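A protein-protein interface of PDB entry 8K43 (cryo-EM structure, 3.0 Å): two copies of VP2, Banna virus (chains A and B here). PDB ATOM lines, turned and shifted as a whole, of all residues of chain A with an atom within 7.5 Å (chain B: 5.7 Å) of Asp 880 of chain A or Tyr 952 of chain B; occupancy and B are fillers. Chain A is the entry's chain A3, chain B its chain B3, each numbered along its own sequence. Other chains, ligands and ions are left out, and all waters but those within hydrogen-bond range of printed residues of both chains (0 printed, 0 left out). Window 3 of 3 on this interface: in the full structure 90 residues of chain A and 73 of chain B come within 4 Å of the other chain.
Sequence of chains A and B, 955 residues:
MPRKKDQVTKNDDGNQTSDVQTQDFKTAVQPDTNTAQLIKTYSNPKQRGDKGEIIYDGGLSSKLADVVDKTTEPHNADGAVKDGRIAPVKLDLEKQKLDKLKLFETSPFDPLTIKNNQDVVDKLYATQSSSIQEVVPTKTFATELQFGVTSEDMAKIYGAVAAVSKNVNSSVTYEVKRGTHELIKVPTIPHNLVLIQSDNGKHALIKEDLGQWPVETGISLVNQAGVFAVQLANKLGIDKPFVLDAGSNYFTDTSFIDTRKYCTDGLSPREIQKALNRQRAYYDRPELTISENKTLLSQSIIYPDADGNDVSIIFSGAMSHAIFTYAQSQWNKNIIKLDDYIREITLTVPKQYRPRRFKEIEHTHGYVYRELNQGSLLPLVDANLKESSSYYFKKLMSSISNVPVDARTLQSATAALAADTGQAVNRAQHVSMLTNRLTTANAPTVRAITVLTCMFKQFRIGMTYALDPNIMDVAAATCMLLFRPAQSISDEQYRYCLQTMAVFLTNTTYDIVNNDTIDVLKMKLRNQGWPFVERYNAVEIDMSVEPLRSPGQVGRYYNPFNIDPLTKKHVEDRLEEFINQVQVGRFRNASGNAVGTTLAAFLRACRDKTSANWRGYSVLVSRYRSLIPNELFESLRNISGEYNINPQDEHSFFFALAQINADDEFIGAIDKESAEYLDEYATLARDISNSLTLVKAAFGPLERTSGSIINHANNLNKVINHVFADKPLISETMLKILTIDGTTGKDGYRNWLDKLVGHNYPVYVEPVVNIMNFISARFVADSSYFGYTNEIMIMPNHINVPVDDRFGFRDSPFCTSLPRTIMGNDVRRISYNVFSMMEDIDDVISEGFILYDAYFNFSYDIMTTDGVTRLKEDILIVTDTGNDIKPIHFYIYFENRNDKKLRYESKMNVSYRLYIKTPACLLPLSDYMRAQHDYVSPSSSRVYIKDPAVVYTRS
The backbone carbonyl oxygen (O) of Met 837 of chain A sits at hydrogen-bond distance from the guanidinium group (NH2) of Arg 354 of chain B, at 2.7 Å. The side-chain hydroxyl (OH) of Tyr 952 of chain B sits at hydrogen-bond distance from the backbone carbonyl oxygen (O) of Asp 880 of chain A, at 3.1 Å. NH1 of Arg 354 of chain B lies within salt-bridge range of OE2 of Glu 839 of chain A (3.5 Å). The backbone NH (N) of Arg 954 of chain B lies close to the side-chain sulfur (SD) of Met 837 of chain A, 3.7 Å away. O of Thr 881 of chain A sits close to OH of Tyr 952 of chain B (3.2 Å).
OG of Ser 836 of chain A touches CB of Arg 954 of chain B, at 3.7 Å. Arg 356 of chain B touches Asp 880 of chain A (CD to OD2, 3.8 Å). CA of Gly 882 of chain A touches NH1 of Arg 954 of chain B, at 3.6 Å.
Asp 880 of chain A touches just these residues of chain B: Arg 356 and Tyr 952. Tyr 952 of chain B touches just these residues of chain A: Asp 880 (3.1 Å) and Thr 881 (3.1 Å). Of the printed residues of chain A, Arg 954 of chain B touches Ser 836, Met 837 and Gly 882. Printed residues of chain B within 4 Å of Ser 836 of chain A: Arg 954. Of the printed residues of chain B, Thr 881 of chain A touches Tyr 952. Of the printed residues of chain B, Met 837 of chain A touches Arg 354 and Arg 954. Of the printed residues of chain A, Arg 356 of chain B touches Asp 880 (3.8 Å). Gln 352 of chain B touches none of the printed residues of chain A. The nearest residue of chain B that does not touch Asp 880 of chain A is Arg 357 of chain B (5.0 Å). The nearest residue of chain A that does not touch Tyr 952 of chain B is Gly 882 of chain A (4.9 Å).
No position is printed for both chains. Of the 8 pairs that touch across the chains among the printed residues, none has its exchanged pair printed and touching as well.
The side-chain hydroxyl (OG1) of Thr 879 of chain A sits at hydrogen-bond distance from the side-chain hydroxyl (OG1) of Thr 881 of chain A, 3.3 Å away. The backbone carbonyl oxygen (O) of Tyr 952 of chain B is in hydrogen-bond range of the backbone NH (N) of Arg 354 of chain B (3.2 Å). N of Asn 883 of chain A is in hydrogen-bond range of O of Ser 836 of chain A (3.1 Å). The backbone NH (N) of Arg 356 of chain B sits at hydrogen-bond distance from the backbone carbonyl oxygen (O) of Val 950 of chain B, 2.5 Å away. The backbone carbonyl oxygen (O) of Gly 882 of chain A sits at hydrogen-bond distance from the side-chain hydroxyl (OG1) of Thr 879 of chain A (2.6 Å).
Of the 9 printed residues of chain A, 6 touch a printed residue of chain B. Hydrophobic or aromatic side chains of chain B that line the printed part of chain A: Tyr 952. Among the printed residues, Asp or Glu carboxylates within 4 Å of a Lys or Arg side-chain nitrogen of the other chain: Glu 839 of chain A with Arg 354 of chain B (3.5 Å).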
ATOM      1  N   SER A 836     -29.952  -8.434  -9.845  1.00  0.00           N
ATOM      2  CA  SER A 836     -29.143  -9.093 -10.863  1.00  0.00           C
ATOM      3  C   SER A 836     -28.613  -8.087 -11.874  1.00  0.00           C
ATOM      4  O   SER A 836     -27.602  -8.336 -12.540  1.00  0.00           O
ATOM      5  CB  SER A 836     -29.962 -10.165 -11.575  1.00  0.00           C
ATOM      6  OG  SER A 836     -30.844  -9.575 -12.513  1.00  0.00           O
ATOM      7  N   MET A 837     -29.288  -6.948 -12.002  1.00  0.00           N
ATOM      8  CA  MET A 837     -29.034  -5.972 -13.054  1.00  0.00           C
ATOM      9  C   MET A 837     -27.921  -4.995 -12.688  1.00  0.00           C
ATOM     10  O   MET A 837     -27.562  -4.147 -13.513  1.00  0.00           O
ATOM     11  CB  MET A 837     -30.323  -5.188 -13.329  1.00  0.00           C
ATOM     12  CG  MET A 837     -31.188  -5.646 -14.520  1.00  0.00           C
ATOM     13  SD  MET A 837     -30.494  -6.479 -15.970  1.00  0.00           S
ATOM     14  CE  MET A 837     -29.175  -5.371 -16.437  1.00  0.00           C
ATOM     15  N   GLU A 839     -24.306  -3.157 -11.059  1.00  0.00           N
ATOM     16  CA  GLU A 839     -22.849  -3.186 -11.075  1.00  0.00           C
ATOM     17  C   GLU A 839     -22.233  -2.724  -9.765  1.00  0.00           C
ATOM     18  O   GLU A 839     -21.060  -3.011  -9.509  1.00  0.00           O
ATOM     19  CB  GLU A 839     -22.304  -2.315 -12.214  1.00  0.00           C
ATOM     20  CG  GLU A 839     -22.606  -2.822 -13.610  1.00  0.00           C
ATOM     21  CD  GLU A 839     -22.113  -1.894 -14.702  1.00  0.00           C
ATOM     22  OE1 GLU A 839     -21.696  -0.754 -14.404  1.00  0.00           O
ATOM     23  OE2 GLU A 839     -22.092  -2.335 -15.863  1.00  0.00           O
ATOM     24  N   VAL A 878     -21.125 -13.637  -9.597  1.00  0.00           N
ATOM     25  CA  VAL A 878     -21.138 -12.408 -10.382  1.00  0.00           C
ATOM     26  C   VAL A 878     -20.527 -12.700 -11.744  1.00  0.00           C
ATOM     27  O   VAL A 878     -19.355 -13.080 -11.839  1.00  0.00           O
ATOM     28  CB  VAL A 878     -20.381 -11.273  -9.678  1.00  0.00           C
ATOM     29  CG1 VAL A 878     -20.359 -10.035 -10.551  1.00  0.00           C
ATOM     30  CG2 VAL A 878     -21.018 -10.964  -8.344  1.00  0.00           C
ATOM     31  N   THR A 879     -21.318 -12.511 -12.793  1.00  0.00           N
ATOM     32  CA  THR A 879     -20.877 -12.673 -14.169  1.00  0.00           C
ATOM     33  C   THR A 879     -20.961 -11.334 -14.885  1.00  0.00           C
ATOM     34  O   THR A 879     -21.431 -10.335 -14.335  1.00  0.00           O
ATOM     35  CB  THR A 879     -21.722 -13.720 -14.907  1.00  0.00           C
ATOM     36  OG1 THR A 879     -23.108 -13.376 -14.803  1.00  0.00           O
ATOM     37  CG2 THR A 879     -21.506 -15.097 -14.310  1.00  0.00           C
ATOM     38  N   ASP A 880     -20.500 -11.319 -16.135  1.00  0.00           N
ATOM     39  CA  ASP A 880     -20.605 -10.103 -16.929  1.00  0.00           C
ATOM     40  C   ASP A 880     -22.019  -9.847 -17.433  1.00  0.00           C
ATOM     41  O   ASP A 880     -22.269  -8.782 -18.007  1.00  0.00           O
ATOM     42  CB  ASP A 880     -19.551 -10.134 -18.058  1.00  0.00           C
ATOM     43  CG  ASP A 880     -19.704 -11.302 -19.048  1.00  0.00           C
ATOM     44  OD1 ASP A 880     -20.600 -12.131 -18.792  1.00  0.00           O
ATOM     45  OD2 ASP A 880     -18.986 -11.328 -20.027  1.00  0.00           O
ATOM     46  N   THR A 881     -22.939 -10.791 -17.241  1.00  0.00           N
ATOM     47  CA  THR A 881     -24.343 -10.575 -17.577  1.00  0.00           C
ATOM     48  C   THR A 881     -25.142 -10.111 -16.360  1.00  0.00           C
ATOM     49  O   THR A 881     -25.747  -9.035 -16.381  1.00  0.00           O
ATOM     50  CB  THR A 881     -24.959 -11.851 -18.156  1.00  0.00           C
ATOM     51  OG1 THR A 881     -25.401 -12.694 -17.087  1.00  0.00           O
ATOM     52  CG2 THR A 881     -23.945 -12.601 -18.998  1.00  0.00           C
ATOM     53  N   GLY A 882     -25.147 -10.906 -15.294  1.00  0.00           N
ATOM     54  CA  GLY A 882     -25.909 -10.546 -14.113  1.00  0.00           C
ATOM     55  C   GLY A 882     -25.443 -11.303 -12.892  1.00  0.00           C
ATOM     56  O   GLY A 882     -24.580 -12.180 -12.961  1.00  0.00           O
ATOM     57  N   ASN A 883     -26.036 -10.946 -11.758  1.00  0.00           N
ATOM     58  CA  ASN A 883     -25.726 -11.556 -10.473  1.00  0.00           C
ATOM     59  C   ASN A 883     -26.837 -12.521 -10.089  1.00  0.00           C
ATOM     60  O   ASN A 883     -28.019 -12.168 -10.149  1.00  0.00           O
ATOM     61  CB  ASN A 883     -25.560 -10.488  -9.392  1.00  0.00           C
ATOM     62  CG  ASN A 883     -24.769  -9.293  -9.869  1.00  0.00           C
ATOM     63  OD1 ASN A 883     -23.602  -9.413 -10.234  1.00  0.00           O
ATOM     64  ND2 ASN A 883     -25.400  -8.128  -9.868  1.00  0.00           N
ATOM     65  N   VAL B 172     -34.470 -11.144 -25.550  1.00  0.00           N
ATOM     66  CA  VAL B 172     -33.796 -11.423 -26.811  1.00  0.00           C
ATOM     67  C   VAL B 172     -32.360 -10.940 -26.707  1.00  0.00           C
ATOM     68  O   VAL B 172     -32.060 -10.012 -25.948  1.00  0.00           O
ATOM     69  CB  VAL B 172     -34.499 -10.749 -28.006  1.00  0.00           C
ATOM     70  CG1 VAL B 172     -35.685 -11.565 -28.443  1.00  0.00           C
ATOM     71  CG2 VAL B 172     -34.926  -9.338 -27.642  1.00  0.00           C
ATOM     72  N   THR B 173     -31.471 -11.572 -27.468  1.00  0.00           N
ATOM     73  CA  THR B 173     -30.072 -11.180 -27.513  1.00  0.00           C
ATOM     74  C   THR B 173     -29.589 -11.184 -28.954  1.00  0.00           C
ATOM     75  O   THR B 173     -29.865 -12.118 -29.711  1.00  0.00           O
ATOM     76  CB  THR B 173     -29.199 -12.107 -26.662  1.00  0.00           C
ATOM     77  OG1 THR B 173     -27.821 -11.896 -26.987  1.00  0.00           O
ATOM     78  CG2 THR B 173     -29.561 -13.561 -26.905  1.00  0.00           C
ATOM     79  N   GLN B 352     -34.538  -1.139 -21.196  1.00  0.00           N
ATOM     80  CA  GLN B 352     -34.048  -2.165 -20.284  1.00  0.00           C
ATOM     81  C   GLN B 352     -32.799  -2.855 -20.818  1.00  0.00           C
ATOM     82  O   GLN B 352     -31.911  -3.213 -20.038  1.00  0.00           O
ATOM     83  CB  GLN B 352     -35.148  -3.188 -20.004  1.00  0.00           C
ATOM     84  CG  GLN B 352     -35.490  -4.075 -21.184  1.00  0.00           C
ATOM     85  CD  GLN B 352     -36.304  -3.355 -22.238  1.00  0.00           C
ATOM     86  OE1 GLN B 352     -36.621  -2.176 -22.095  1.00  0.00           O
ATOM     87  NE2 GLN B 352     -36.647  -4.065 -23.306  1.00  0.00           N
ATOM     88  N   TYR B 353     -32.709  -3.046 -22.131  1.00  0.00           N
ATOM     89  CA  TYR B 353     -31.562  -3.719 -22.718  1.00  0.00           C
ATOM     90  C   TYR B 353     -30.334  -2.818 -22.678  1.00  0.00           C
ATOM     91  O   TYR B 353     -30.426  -1.598 -22.835  1.00  0.00           O
ATOM     92  CB  TYR B 353     -31.854  -4.113 -24.166  1.00  0.00           C
ATOM     93  CG  TYR B 353     -32.953  -5.135 -24.343  1.00  0.00           C
ATOM     94  CD1 TYR B 353     -34.283  -4.777 -24.201  1.00  0.00           C
ATOM     95  CD2 TYR B 353     -32.663  -6.448 -24.673  1.00  0.00           C
ATOM     96  CE1 TYR B 353     -35.291  -5.697 -24.368  1.00  0.00           C
ATOM     97  CE2 TYR B 353     -33.668  -7.378 -24.843  1.00  0.00           C
ATOM     98  CZ  TYR B 353     -34.979  -6.996 -24.688  1.00  0.00           C
ATOM     99  OH  TYR B 353     -35.991  -7.913 -24.854  1.00  0.00           O
ATOM    100  N   ARG B 354     -29.174  -3.429 -22.467  1.00  0.00           N
ATOM    101  CA  ARG B 354     -27.916  -2.707 -22.531  1.00  0.00           C
ATOM    102  C   ARG B 354     -26.853  -3.618 -23.123  1.00  0.00           C
ATOM    103  O   ARG B 354     -26.948  -4.844 -22.998  1.00  0.00           O
ATOM    104  CB  ARG B 354     -27.442  -2.233 -21.152  1.00  0.00           C
ATOM    105  CG  ARG B 354     -27.447  -3.283 -20.079  1.00  0.00           C
ATOM    106  CD  ARG B 354     -26.669  -2.721 -18.923  1.00  0.00           C
ATOM    107  NE  ARG B 354     -26.910  -3.389 -17.656  1.00  0.00           N
ATOM    108  CZ  ARG B 354     -25.954  -3.983 -16.959  1.00  0.00           C
ATOM    109  NH1 ARG B 354     -24.704  -4.022 -17.395  1.00  0.00           N
ATOM    110  NH2 ARG B 354     -26.249  -4.536 -15.789  1.00  0.00           N
ATOM    111  N   PRO B 355     -25.829  -3.055 -23.756  1.00  0.00           N
ATOM    112  CA  PRO B 355     -24.758  -3.888 -24.307  1.00  0.00           C
ATOM    113  C   PRO B 355     -23.873  -4.492 -23.228  1.00  0.00           C
ATOM    114  O   PRO B 355     -23.760  -3.979 -22.114  1.00  0.00           O
ATOM    115  CB  PRO B 355     -23.967  -2.910 -25.183  1.00  0.00           C
ATOM    116  CG  PRO B 355     -24.213  -1.591 -24.573  1.00  0.00           C
ATOM    117  CD  PRO B 355     -25.622  -1.628 -24.063  1.00  0.00           C
ATOM    118  N   ARG B 356     -23.243  -5.607 -23.585  1.00  0.00           N
ATOM    119  CA  ARG B 356     -22.282  -6.266 -22.717  1.00  0.00           C
ATOM    120  C   ARG B 356     -20.962  -5.506 -22.718  1.00  0.00           C
ATOM    121  O   ARG B 356     -20.669  -4.728 -23.630  1.00  0.00           O
ATOM    122  CB  ARG B 356     -22.053  -7.708 -23.168  1.00  0.00           C
ATOM    123  CG  ARG B 356     -21.656  -8.666 -22.061  1.00  0.00           C
ATOM    124  CD  ARG B 356     -21.454 -10.075 -22.597  1.00  0.00           C
ATOM    125  NE  ARG B 356     -20.450 -10.118 -23.652  1.00  0.00           N
ATOM    126  CZ  ARG B 356     -20.270 -11.141 -24.475  1.00  0.00           C
ATOM    127  NH1 ARG B 356     -21.011 -12.234 -24.394  1.00  0.00           N
ATOM    128  NH2 ARG B 356     -19.322 -11.068 -25.404  1.00  0.00           N
ATOM    129  N   ARG B 357     -20.160  -5.740 -21.682  1.00  0.00           N
ATOM    130  CA  ARG B 357     -18.890  -5.044 -21.543  1.00  0.00           C
ATOM    131  C   ARG B 357     -17.766  -5.812 -22.227  1.00  0.00           C
ATOM    132  O   ARG B 357     -17.709  -7.043 -22.171  1.00  0.00           O
ATOM    133  CB  ARG B 357     -18.551  -4.840 -20.067  1.00  0.00           C
ATOM    134  CG  ARG B 357     -19.707  -4.330 -19.232  1.00  0.00           C
ATOM    135  CD  ARG B 357     -19.562  -2.845 -18.954  1.00  0.00           C
ATOM    136  NE  ARG B 357     -18.327  -2.545 -18.240  1.00  0.00           N
ATOM    137  CZ  ARG B 357     -17.625  -1.431 -18.394  1.00  0.00           C
ATOM    138  NH1 ARG B 357     -18.011  -0.480 -19.229  1.00  0.00           N
ATOM    139  NH2 ARG B 357     -16.508  -1.266 -17.692  1.00  0.00           N
ATOM    140  N   VAL B 950     -22.673  -7.041 -27.711  1.00  0.00           N
ATOM    141  CA  VAL B 950     -23.733  -7.997 -27.416  1.00  0.00           C
ATOM    142  C   VAL B 950     -24.739  -7.334 -26.488  1.00  0.00           C
ATOM    143  O   VAL B 950     -24.361  -6.772 -25.456  1.00  0.00           O
ATOM    144  CB  VAL B 950     -23.174  -9.285 -26.785  1.00  0.00           C
ATOM    145  CG1 VAL B 950     -24.287 -10.296 -26.576  1.00  0.00           C
ATOM    146  CG2 VAL B 950     -22.083  -9.866 -27.662  1.00  0.00           C
ATOM    147  N   VAL B 951     -26.017  -7.418 -26.850  1.00  0.00           N
ATOM    148  CA  VAL B 951     -27.097  -6.754 -26.128  1.00  0.00           C
ATOM    149  C   VAL B 951     -27.944  -7.805 -25.424  1.00  0.00           C
ATOM    150  O   VAL B 951     -28.227  -8.868 -25.989  1.00  0.00           O
ATOM    151  CB  VAL B 951     -27.955  -5.898 -27.076  1.00  0.00           C
ATOM    152  CG1 VAL B 951     -29.063  -5.218 -26.307  1.00  0.00           C
ATOM    153  CG2 VAL B 951     -27.091  -4.875 -27.780  1.00  0.00           C
ATOM    154  N   TYR B 952     -28.349  -7.504 -24.192  1.00  0.00           N
ATOM    155  CA  TYR B 952     -29.037  -8.467 -23.346  1.00  0.00           C
ATOM    156  C   TYR B 952     -29.775  -7.720 -22.245  1.00  0.00           C
ATOM    157  O   TYR B 952     -29.531  -6.537 -21.999  1.00  0.00           O
ATOM    158  CB  TYR B 952     -28.050  -9.465 -22.740  1.00  0.00           C
ATOM    159  CG  TYR B 952     -27.186  -8.848 -21.670  1.00  0.00           C
ATOM    160  CD1 TYR B 952     -26.209  -7.918 -21.992  1.00  0.00           C
ATOM    161  CD2 TYR B 952     -27.358  -9.177 -20.338  1.00  0.00           C
ATOM    162  CE1 TYR B 952     -25.426  -7.344 -21.017  1.00  0.00           C
ATOM    163  CE2 TYR B 952     -26.580  -8.608 -19.360  1.00  0.00           C
ATOM    164  CZ  TYR B 952     -25.616  -7.692 -19.704  1.00  0.00           C
ATOM    165  OH  TYR B 952     -24.833  -7.121 -18.728  1.00  0.00           O
ATOM    166  N   THR B 953     -30.681  -8.430 -21.580  1.00  0.00           N
ATOM    167  CA  THR B 953     -31.358  -7.904 -20.403  1.00  0.00           C
ATOM    168  C   THR B 953     -31.845  -9.073 -19.562  1.00  0.00           C
ATOM    169  O   THR B 953     -31.955 -10.203 -20.045  1.00  0.00           O
ATOM    170  CB  THR B 953     -32.526  -6.987 -20.771  1.00  0.00           C
ATOM    171  OG1 THR B 953     -33.038  -6.370 -19.584  1.00  0.00           O
ATOM    172  CG2 THR B 953     -33.635  -7.785 -21.424  1.00  0.00           C
ATOM    173  N   ARG B 954     -32.130  -8.790 -18.292  1.00  0.00           N
ATOM    174  CA  ARG B 954     -32.588  -9.811 -17.362  1.00  0.00           C
ATOM    175  C   ARG B 954     -34.007  -9.589 -16.863  1.00  0.00           C
ATOM    176  O   ARG B 954     -34.491 -10.387 -16.052  1.00  0.00           O
ATOM    177  CB  ARG B 954     -31.639  -9.909 -16.160  1.00  0.00           C
ATOM    178  CG  ARG B 954     -30.239 -10.350 -16.522  1.00  0.00           C
ATOM    179  CD  ARG B 954     -30.148 -11.860 -16.607  1.00  0.00           C
ATOM    180  NE  ARG B 954     -30.646 -12.518 -15.407  1.00  0.00           N
ATOM    181  CZ  ARG B 954     -29.875 -13.006 -14.446  1.00  0.00           C
ATOM    182  NH1 ARG B 954     -28.556 -12.924 -14.511  1.00  0.00           N
ATOM    183  NH2 ARG B 954     -30.438 -13.596 -13.396  1.00  0.00           N
